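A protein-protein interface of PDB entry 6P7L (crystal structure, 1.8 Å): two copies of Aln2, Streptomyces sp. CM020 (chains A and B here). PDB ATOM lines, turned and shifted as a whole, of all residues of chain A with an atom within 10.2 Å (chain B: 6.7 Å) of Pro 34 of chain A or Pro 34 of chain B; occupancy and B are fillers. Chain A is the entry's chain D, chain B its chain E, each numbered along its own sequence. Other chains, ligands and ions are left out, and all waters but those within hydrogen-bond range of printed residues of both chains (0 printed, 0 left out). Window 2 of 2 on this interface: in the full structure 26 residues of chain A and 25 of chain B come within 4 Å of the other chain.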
ATOM      1  N   LYS A  30     -32.170  11.087  15.432  1.00  0.00           N
ATOM      2  CA  LYS A  30     -31.992   9.640  15.471  1.00  0.00           C
ATOM      3  C   LYS A  30     -30.532   9.301  15.157  1.00  0.00           C
ATOM      4  O   LYS A  30     -29.865   8.772  16.012  1.00  0.00           O
ATOM      5  CB  LYS A  30     -32.923   8.925  14.501  1.00  0.00           C
ATOM      6  CG  LYS A  30     -32.974   7.432  14.714  1.00  0.00           C
ATOM      7  CD  LYS A  30     -34.385   6.871  14.841  1.00  0.00           C
ATOM      8  CE  LYS A  30     -34.372   5.352  14.717  1.00  0.00           C
ATOM      9  NZ  LYS A  30     -33.113   4.784  15.308  1.00  0.00           N
ATOM     10  N   LEU A  31     -30.033   9.612  13.958  1.00  0.00           N
ATOM     11  CA  LEU A  31     -28.631   9.296  13.648  1.00  0.00           C
ATOM     12  C   LEU A  31     -27.703  10.219  14.444  1.00  0.00           C
ATOM     13  O   LEU A  31     -27.975  11.418  14.554  1.00  0.00           O
ATOM     14  CB  LEU A  31     -28.354   9.451  12.154  1.00  0.00           C
ATOM     15  CG  LEU A  31     -29.066   8.442  11.233  1.00  0.00           C
ATOM     16  CD1 LEU A  31     -28.994   8.786   9.768  1.00  0.00           C
ATOM     17  CD2 LEU A  31     -28.458   7.065  11.489  1.00  0.00           C
ATOM     18  N   PRO A  32     -26.601   9.684  14.984  1.00  0.00           N
ATOM     19  CA  PRO A  32     -25.640  10.512  15.720  1.00  0.00           C
ATOM     20  C   PRO A  32     -24.813  11.343  14.757  1.00  0.00           C
ATOM     21  O   PRO A  32     -24.580  10.948  13.613  1.00  0.00           O
ATOM     22  CB  PRO A  32     -24.762   9.478  16.423  1.00  0.00           C
ATOM     23  CG  PRO A  32     -24.694   8.351  15.433  1.00  0.00           C
ATOM     24  CD  PRO A  32     -26.094   8.310  14.790  1.00  0.00           C
ATOM     25  N   SER A  33     -24.338  12.487  15.254  1.00  0.00           N
ATOM     26  CA  SER A  33     -23.439  13.288  14.432  1.00  0.00           C
ATOM     27  C   SER A  33     -22.180  12.476  14.133  1.00  0.00           C
ATOM     28  O   SER A  33     -21.800  11.585  14.912  1.00  0.00           O
ATOM     29  CB  SER A  33     -23.070  14.600  15.120  1.00  0.00           C
ATOM     30  OG  SER A  33     -22.232  14.315  16.233  1.00  0.00           O
ATOM     31  N   PRO A  34     -21.476  12.764  13.030  1.00  0.00           N
ATOM     32  CA  PRO A  34     -20.214  12.046  12.823  1.00  0.00           C
ATOM     33  C   PRO A  34     -19.222  12.288  13.958  1.00  0.00           C
ATOM     34  O   PRO A  34     -18.464  11.370  14.310  1.00  0.00           O
ATOM     35  CB  PRO A  34     -19.721  12.581  11.464  1.00  0.00           C
ATOM     36  CG  PRO A  34     -20.989  12.960  10.757  1.00  0.00           C
ATOM     37  CD  PRO A  34     -21.832  13.587  11.854  1.00  0.00           C
ATOM     38  N   GLU A  35     -19.221  13.490  14.554  1.00  0.00           N
ATOM     39  CA  GLU A  35     -18.304  13.747  15.659  1.00  0.00           C
ATOM     40  C   GLU A  35     -18.606  12.817  16.819  1.00  0.00           C
ATOM     41  O   GLU A  35     -17.700  12.224  17.417  1.00  0.00           O
ATOM     42  CB  GLU A  35     -18.411  15.202  16.082  1.00  0.00           C
ATOM     43  CG  GLU A  35     -17.660  16.162  15.171  1.00  0.00           C
ATOM     44  CD  GLU A  35     -18.382  16.492  13.855  1.00  0.00           C
ATOM     45  OE1 GLU A  35     -19.589  16.142  13.631  1.00  0.00           O
ATOM     46  OE2 GLU A  35     -17.709  17.154  13.028  1.00  0.00           O
ATOM     47  N   LEU A  36     -19.882  12.679  17.156  1.00  0.00           N
ATOM     48  CA  LEU A  36     -20.244  11.791  18.260  1.00  0.00           C
ATOM     49  C   LEU A  36     -19.879  10.345  17.934  1.00  0.00           C
ATOM     50  O   LEU A  36     -19.307   9.633  18.770  1.00  0.00           O
ATOM     51  CB  LEU A  36     -21.741  11.909  18.557  1.00  0.00           C
ATOM     52  CG  LEU A  36     -22.211  10.928  19.640  1.00  0.00           C
ATOM     53  CD1 LEU A  36     -21.468  11.110  20.950  1.00  0.00           C
ATOM     54  CD2 LEU A  36     -23.687  11.100  19.852  1.00  0.00           C
ATOM     55  N   TYR A  37     -20.187   9.899  16.718  1.00  0.00           N
ATOM     56  CA  TYR A  37     -19.863   8.527  16.333  1.00  0.00           C
ATOM     57  C   TYR A  37     -18.374   8.253  16.495  1.00  0.00           C
ATOM     58  O   TYR A  37     -17.983   7.234  17.074  1.00  0.00           O
ATOM     59  CB  TYR A  37     -20.314   8.249  14.889  1.00  0.00           C
ATOM     60  CG  TYR A  37     -20.082   6.801  14.513  1.00  0.00           C
ATOM     61  CD1 TYR A  37     -21.000   5.831  14.863  1.00  0.00           C
ATOM     62  CD2 TYR A  37     -18.938   6.407  13.861  1.00  0.00           C
ATOM     63  CE1 TYR A  37     -20.784   4.512  14.589  1.00  0.00           C
ATOM     64  CE2 TYR A  37     -18.728   5.075  13.533  1.00  0.00           C
ATOM     65  CZ  TYR A  37     -19.665   4.137  13.917  1.00  0.00           C
ATOM     66  OH  TYR A  37     -19.494   2.803  13.680  1.00  0.00           O
ATOM     67  N   VAL A  38     -17.530   9.148  15.987  1.00  0.00           N
ATOM     68  CA  VAL A  38     -16.087   8.959  16.099  1.00  0.00           C
ATOM     69  C   VAL A  38     -15.650   8.932  17.550  1.00  0.00           C
ATOM     70  O   VAL A  38     -14.834   8.085  17.948  1.00  0.00           O
ATOM     71  CB  VAL A  38     -15.323  10.035  15.313  1.00  0.00           C
ATOM     72  CG1 VAL A  38     -13.807   9.990  15.619  1.00  0.00           C
ATOM     73  CG2 VAL A  38     -15.598   9.831  13.837  1.00  0.00           C
ATOM     74  N   GLU A  39     -16.174   9.863  18.348  1.00  0.00           N
ATOM     75  CA  GLU A  39     -15.820   9.944  19.761  1.00  0.00           C
ATOM     76  C   GLU A  39     -16.154   8.644  20.481  1.00  0.00           C
ATOM     77  O   GLU A  39     -15.371   8.182  21.327  1.00  0.00           O
ATOM     78  CB  GLU A  39     -16.542  11.112  20.420  1.00  0.00           C
ATOM     79  CG  GLU A  39     -16.135  11.365  21.854  1.00  0.00           C
ATOM     80  CD  GLU A  39     -16.846  12.572  22.469  1.00  0.00           C
ATOM     81  OE1 GLU A  39     -17.879  13.042  21.931  1.00  0.00           O
ATOM     82  OE2 GLU A  39     -16.362  13.060  23.505  1.00  0.00           O
ATOM     83  N   VAL A  40     -17.307   8.042  20.152  1.00  0.00           N
ATOM     84  CA  VAL A  40     -17.695   6.766  20.751  1.00  0.00           C
ATOM     85  C   VAL A  40     -16.732   5.650  20.347  1.00  0.00           C
ATOM     86  O   VAL A  40     -16.307   4.860  21.200  1.00  0.00           O
ATOM     87  CB  VAL A  40     -19.160   6.432  20.399  1.00  0.00           C
ATOM     88  CG1 VAL A  40     -19.501   5.008  20.794  1.00  0.00           C
ATOM     89  CG2 VAL A  40     -20.081   7.394  21.097  1.00  0.00           C
ATOM     90  N   THR A  41     -16.331   5.577  19.063  1.00  0.00           N
ATOM     91  CA  THR A  41     -15.379   4.523  18.690  1.00  0.00           C
ATOM     92  C   THR A  41     -14.058   4.679  19.443  1.00  0.00           C
ATOM     93  O   THR A  41     -13.405   3.686  19.810  1.00  0.00           O
ATOM     94  CB  THR A  41     -15.077   4.492  17.183  1.00  0.00           C
ATOM     95  OG1 THR A  41     -14.191   5.563  16.802  1.00  0.00           O
ATOM     96  CG2 THR A  41     -16.358   4.481  16.347  1.00  0.00           C
ATOM     97  N   GLN A  42     -13.607   5.920  19.621  1.00  0.00           N
ATOM     98  CA  GLN A  42     -12.339   6.156  20.304  1.00  0.00           C
ATOM     99  C   GLN A  42     -12.458   5.887  21.797  1.00  0.00           C
ATOM    100  O   GLN A  42     -11.532   5.347  22.418  1.00  0.00           O
ATOM    101  CB  GLN A  42     -11.872   7.591  20.062  1.00  0.00           C
ATOM    102  CG  GLN A  42     -11.614   7.893  18.580  1.00  0.00           C
ATOM    103  CD  GLN A  42     -10.636   6.924  17.977  1.00  0.00           C
ATOM    104  OE1 GLN A  42      -9.410   7.012  18.193  1.00  0.00           O
ATOM    105  NE2 GLN A  42     -11.173   5.931  17.288  1.00  0.00           N
ATOM    106  N   VAL A 108     -25.608   3.629  17.804  1.00  0.00           N
ATOM    107  CA  VAL A 108     -25.244   4.809  18.579  1.00  0.00           C
ATOM    108  C   VAL A 108     -26.368   5.830  18.430  1.00  0.00           C
ATOM    109  O   VAL A 108     -26.703   6.238  17.315  1.00  0.00           O
ATOM    110  CB  VAL A 108     -23.908   5.427  18.126  1.00  0.00           C
ATOM    111  CG1 VAL A 108     -23.623   6.691  18.941  1.00  0.00           C
ATOM    112  CG2 VAL A 108     -22.762   4.429  18.236  1.00  0.00           C
ATOM    113  N   GLU A 110     -28.050   9.524  20.367  1.00  0.00           N
ATOM    114  CA  GLU A 110     -28.057  10.560  21.394  1.00  0.00           C
ATOM    115  C   GLU A 110     -29.496  10.911  21.774  1.00  0.00           C
ATOM    116  O   GLU A 110     -30.312  11.270  20.917  1.00  0.00           O
ATOM    117  CB  GLU A 110     -27.341  11.821  20.916  1.00  0.00           C
ATOM    118  CG  GLU A 110     -27.214  12.906  21.990  1.00  0.00           C
ATOM    119  CD  GLU A 110     -26.453  14.127  21.514  1.00  0.00           C
ATOM    120  OE1 GLU A 110     -25.934  14.102  20.361  1.00  0.00           O
ATOM    121  OE2 GLU A 110     -26.370  15.100  22.298  1.00  0.00           O
ATOM    122  N   ARG A 147     -21.782  12.685  29.272  1.00  0.00           N
ATOM    123  CA  ARG A 147     -20.694  13.639  29.142  1.00  0.00           C
ATOM    124  C   ARG A 147     -20.447  14.290  30.496  1.00  0.00           C
ATOM    125  O   ARG A 147     -21.378  14.783  31.136  1.00  0.00           O
ATOM    126  CB  ARG A 147     -21.013  14.686  28.073  1.00  0.00           C
ATOM    127  CG  ARG A 147     -19.786  15.395  27.549  1.00  0.00           C
ATOM    128  CD  ARG A 147     -20.084  16.154  26.271  1.00  0.00           C
ATOM    129  NE  ARG A 147     -20.493  15.291  25.160  1.00  0.00           N
ATOM    130  CZ  ARG A 147     -19.650  14.619  24.373  1.00  0.00           C
ATOM    131  NH1 ARG A 147     -18.339  14.688  24.549  1.00  0.00           N
ATOM    132  NH2 ARG A 147     -20.118  13.891  23.377  1.00  0.00           N
ATOM    133  N   LEU A 152     -16.818  11.953  27.396  1.00  0.00           N
ATOM    134  CA  LEU A 152     -17.701  10.806  27.499  1.00  0.00           C
ATOM    135  C   LEU A 152     -17.185   9.870  28.579  1.00  0.00           C
ATOM    136  O   LEU A 152     -15.974   9.624  28.690  1.00  0.00           O
ATOM    137  CB  LEU A 152     -17.789  10.027  26.193  1.00  0.00           C
ATOM    138  CG  LEU A 152     -18.733  10.541  25.115  1.00  0.00           C
ATOM    139  CD1 LEU A 152     -18.651   9.578  23.922  1.00  0.00           C
ATOM    140  CD2 LEU A 152     -20.145  10.718  25.602  1.00  0.00           C
ATOM    141  N   PRO B  32     -16.684   8.427   0.931  1.00  0.00           N
ATOM    142  CA  PRO B  32     -18.029   8.816   1.351  1.00  0.00           C
ATOM    143  C   PRO B  32     -17.968   9.963   2.358  1.00  0.00           C
ATOM    144  O   PRO B  32     -16.994  10.106   3.089  1.00  0.00           O
ATOM    145  CB  PRO B  32     -18.575   7.551   2.006  1.00  0.00           C
ATOM    146  CG  PRO B  32     -17.366   6.964   2.653  1.00  0.00           C
ATOM    147  CD  PRO B  32     -16.192   7.279   1.731  1.00  0.00           C
ATOM    148  N   SER B  33     -19.016  10.787   2.385  1.00  0.00           N
ATOM    149  CA  SER B  33     -19.105  11.807   3.425  1.00  0.00           C
ATOM    150  C   SER B  33     -19.187  11.126   4.793  1.00  0.00           C
ATOM    151  O   SER B  33     -19.701   9.998   4.907  1.00  0.00           O
ATOM    152  CB  SER B  33     -20.339  12.678   3.236  1.00  0.00           C
ATOM    153  OG  SER B  33     -21.508  11.897   3.517  1.00  0.00           O
ATOM    154  N   PRO B  34     -18.736  11.799   5.855  1.00  0.00           N
ATOM    155  CA  PRO B  34     -18.858  11.176   7.185  1.00  0.00           C
ATOM    156  C   PRO B  34     -20.313  10.879   7.545  1.00  0.00           C
ATOM    157  O   PRO B  34     -20.593   9.859   8.184  1.00  0.00           O
ATOM    158  CB  PRO B  34     -18.211  12.204   8.131  1.00  0.00           C
ATOM    159  CG  PRO B  34     -17.235  12.995   7.244  1.00  0.00           C
ATOM    160  CD  PRO B  34     -17.981  13.076   5.895  1.00  0.00           C
ATOM    161  N   GLU B  35     -21.254  11.742   7.135  1.00  0.00           N
ATOM    162  CA  GLU B  35     -22.664  11.466   7.415  1.00  0.00           C
ATOM    163  C   GLU B  35     -23.114  10.172   6.751  1.00  0.00           C
ATOM    164  O   GLU B  35     -23.842   9.362   7.354  1.00  0.00           O
ATOM    165  CB  GLU B  35     -23.516  12.639   6.954  1.00  0.00           C
ATOM    166  CG  GLU B  35     -23.205  13.939   7.692  1.00  0.00           C
ATOM    167  CD  GLU B  35     -21.945  14.667   7.157  1.00  0.00           C
ATOM    168  OE1 GLU B  35     -21.408  14.332   6.078  1.00  0.00           O
ATOM    169  OE2 GLU B  35     -21.479  15.599   7.836  1.00  0.00           O
ATOM    170  N   LEU B  36     -22.731   9.975   5.494  1.00  0.00           N
ATOM    171  CA  LEU B  36     -23.115   8.731   4.817  1.00  0.00           C
ATOM    172  C   LEU B  36     -22.480   7.528   5.495  1.00  0.00           C
ATOM    173  O   LEU B  36     -23.120   6.502   5.704  1.00  0.00           O
ATOM    174  CB  LEU B  36     -22.719   8.753   3.342  1.00  0.00           C
ATOM    175  CG  LEU B  36     -23.045   7.434   2.585  1.00  0.00           C
ATOM    176  CD1 LEU B  36     -24.566   7.276   2.568  1.00  0.00           C
ATOM    177  CD2 LEU B  36     -22.502   7.442   1.204  1.00  0.00           C
ATOM    178  N   TYR B  37     -21.197   7.628   5.838  1.00  0.00           N
ATOM    179  CA  TYR B  37     -20.535   6.500   6.474  1.00  0.00           C
ATOM    180  C   TYR B  37     -21.241   6.122   7.775  1.00  0.00           C
ATOM    181  O   TYR B  37     -21.532   4.940   8.033  1.00  0.00           O
ATOM    182  CB  TYR B  37     -19.057   6.849   6.695  1.00  0.00           C
ATOM    183  CG  TYR B  37     -18.319   5.671   7.226  1.00  0.00           C
ATOM    184  CD1 TYR B  37     -17.810   4.718   6.370  1.00  0.00           C
ATOM    185  CD2 TYR B  37     -18.149   5.502   8.588  1.00  0.00           C
ATOM    186  CE1 TYR B  37     -17.151   3.622   6.856  1.00  0.00           C
ATOM    187  CE2 TYR B  37     -17.502   4.393   9.079  1.00  0.00           C
ATOM    188  CZ  TYR B  37     -16.989   3.477   8.197  1.00  0.00           C
ATOM    189  OH  TYR B  37     -16.331   2.372   8.686  1.00  0.00           O
ATOM    190  N   VAL B  38     -21.538   7.113   8.603  1.00  0.00           N
ATOM    191  CA  VAL B  38     -22.232   6.831   9.855  1.00  0.00           C
ATOM    192  C   VAL B  38     -23.588   6.189   9.570  1.00  0.00           C
ATOM    193  O   VAL B  38     -23.963   5.173  10.174  1.00  0.00           O
ATOM    194  CB  VAL B  38     -22.375   8.117  10.681  1.00  0.00           C
ATOM    195  CG1 VAL B  38     -23.278   7.910  11.856  1.00  0.00           C
ATOM    196  CG2 VAL B  38     -20.986   8.556  11.139  1.00  0.00           C
ATOM    197  N   GLU B  39     -24.316   6.735   8.600  1.00  0.00           N
ATOM    198  CA  GLU B  39     -25.633   6.193   8.281  1.00  0.00           C
ATOM    199  C   GLU B  39     -25.546   4.726   7.874  1.00  0.00           C
ATOM    200  O   GLU B  39     -26.404   3.913   8.246  1.00  0.00           O
ATOM    201  CB  GLU B  39     -26.282   7.019   7.170  1.00  0.00           C
ATOM    202  CG  GLU B  39     -27.681   6.575   6.843  1.00  0.00           C
ATOM    203  CD  GLU B  39     -28.340   7.453   5.818  1.00  0.00           C
ATOM    204  OE1 GLU B  39     -27.614   8.119   5.059  1.00  0.00           O
ATOM    205  OE2 GLU B  39     -29.584   7.463   5.763  1.00  0.00           O
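Of the printed residues of chain B, Leu 31 of chain A touches Glu 39 (3.9 Å). Of the printed residues of chain B, Pro 32 of chain A touches Val 38 (3.7 Å). Glu 35 of chain A touches none of the printed residues of chain B. Of the printed residues of chain B, Tyr 37 of chain A touches Val 38. No residue of chain A comes within 4 Å of Ser 33 of chain B. Val 38 of chain B touches three residues of chain A. Printed residues of chain A within 4 Å of Glu 39 of chain B: Leu 31 (3.9 Å). The nearest printed residue of chain B that does not touch Pro 32 of chain A is Glu 35 of chain B (6.5 Å).
Printed residues of chain A that touch a printed residue of chain B: Leu 31, Pro 32, Pro 34 and Tyr 37. Hydrophobic or aromatic side chains of chain A within 4 Å of the printed part of chain B: Leu 31, Pro 32, Pro 34 and Tyr 37. Along chain A the printed residues that touch a printed residue of chain B span positions 31 to 37. Of the 8 printed residues of chain B, 4 touch a printed residue of chain A. Hydrophobic or aromatic side chains of chain B within 4 Å of the printed part of chain A: Pro 34 and Val 38. Among the printed residues, 6 pairs touch across the chains.
Pro 32 of chain A touches Val 38 of chain B, but with the chains exchanged Val 38 of chain A does not touch Pro 32 of chain B (10.8 Å). Pro 34 of chain A touches Glu 35 of chain B, but with the chains exchanged Glu 35 of chain A does not touch Pro 34 of chain B (6.6 Å). Pro 34 of chain A touches Val 38 of chain B, but with the chains exchanged Val 38 of chain A does not touch Pro 34 of chain B (6.7 Å). Tyr 37 of chain A touches Val 38 of chain B, but with the chains exchanged Val 38 of chain A does not touch Tyr 37 of chain B (7.3 Å). 8 positions are printed for both chains.
Among the printed residues, merely in contact across the chains: Leu 31 of chain A with Glu 39 of chain B, Pro 32 of chain A with Val 38 of chain B, Pro 34 of chain A with Pro 34 of chain B, Pro 34 of chain A with Glu 35 of chain B, Pro 34 of chain A with Val 38 of chain B and Tyr 37 of chain A with Val 38 of chain B.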
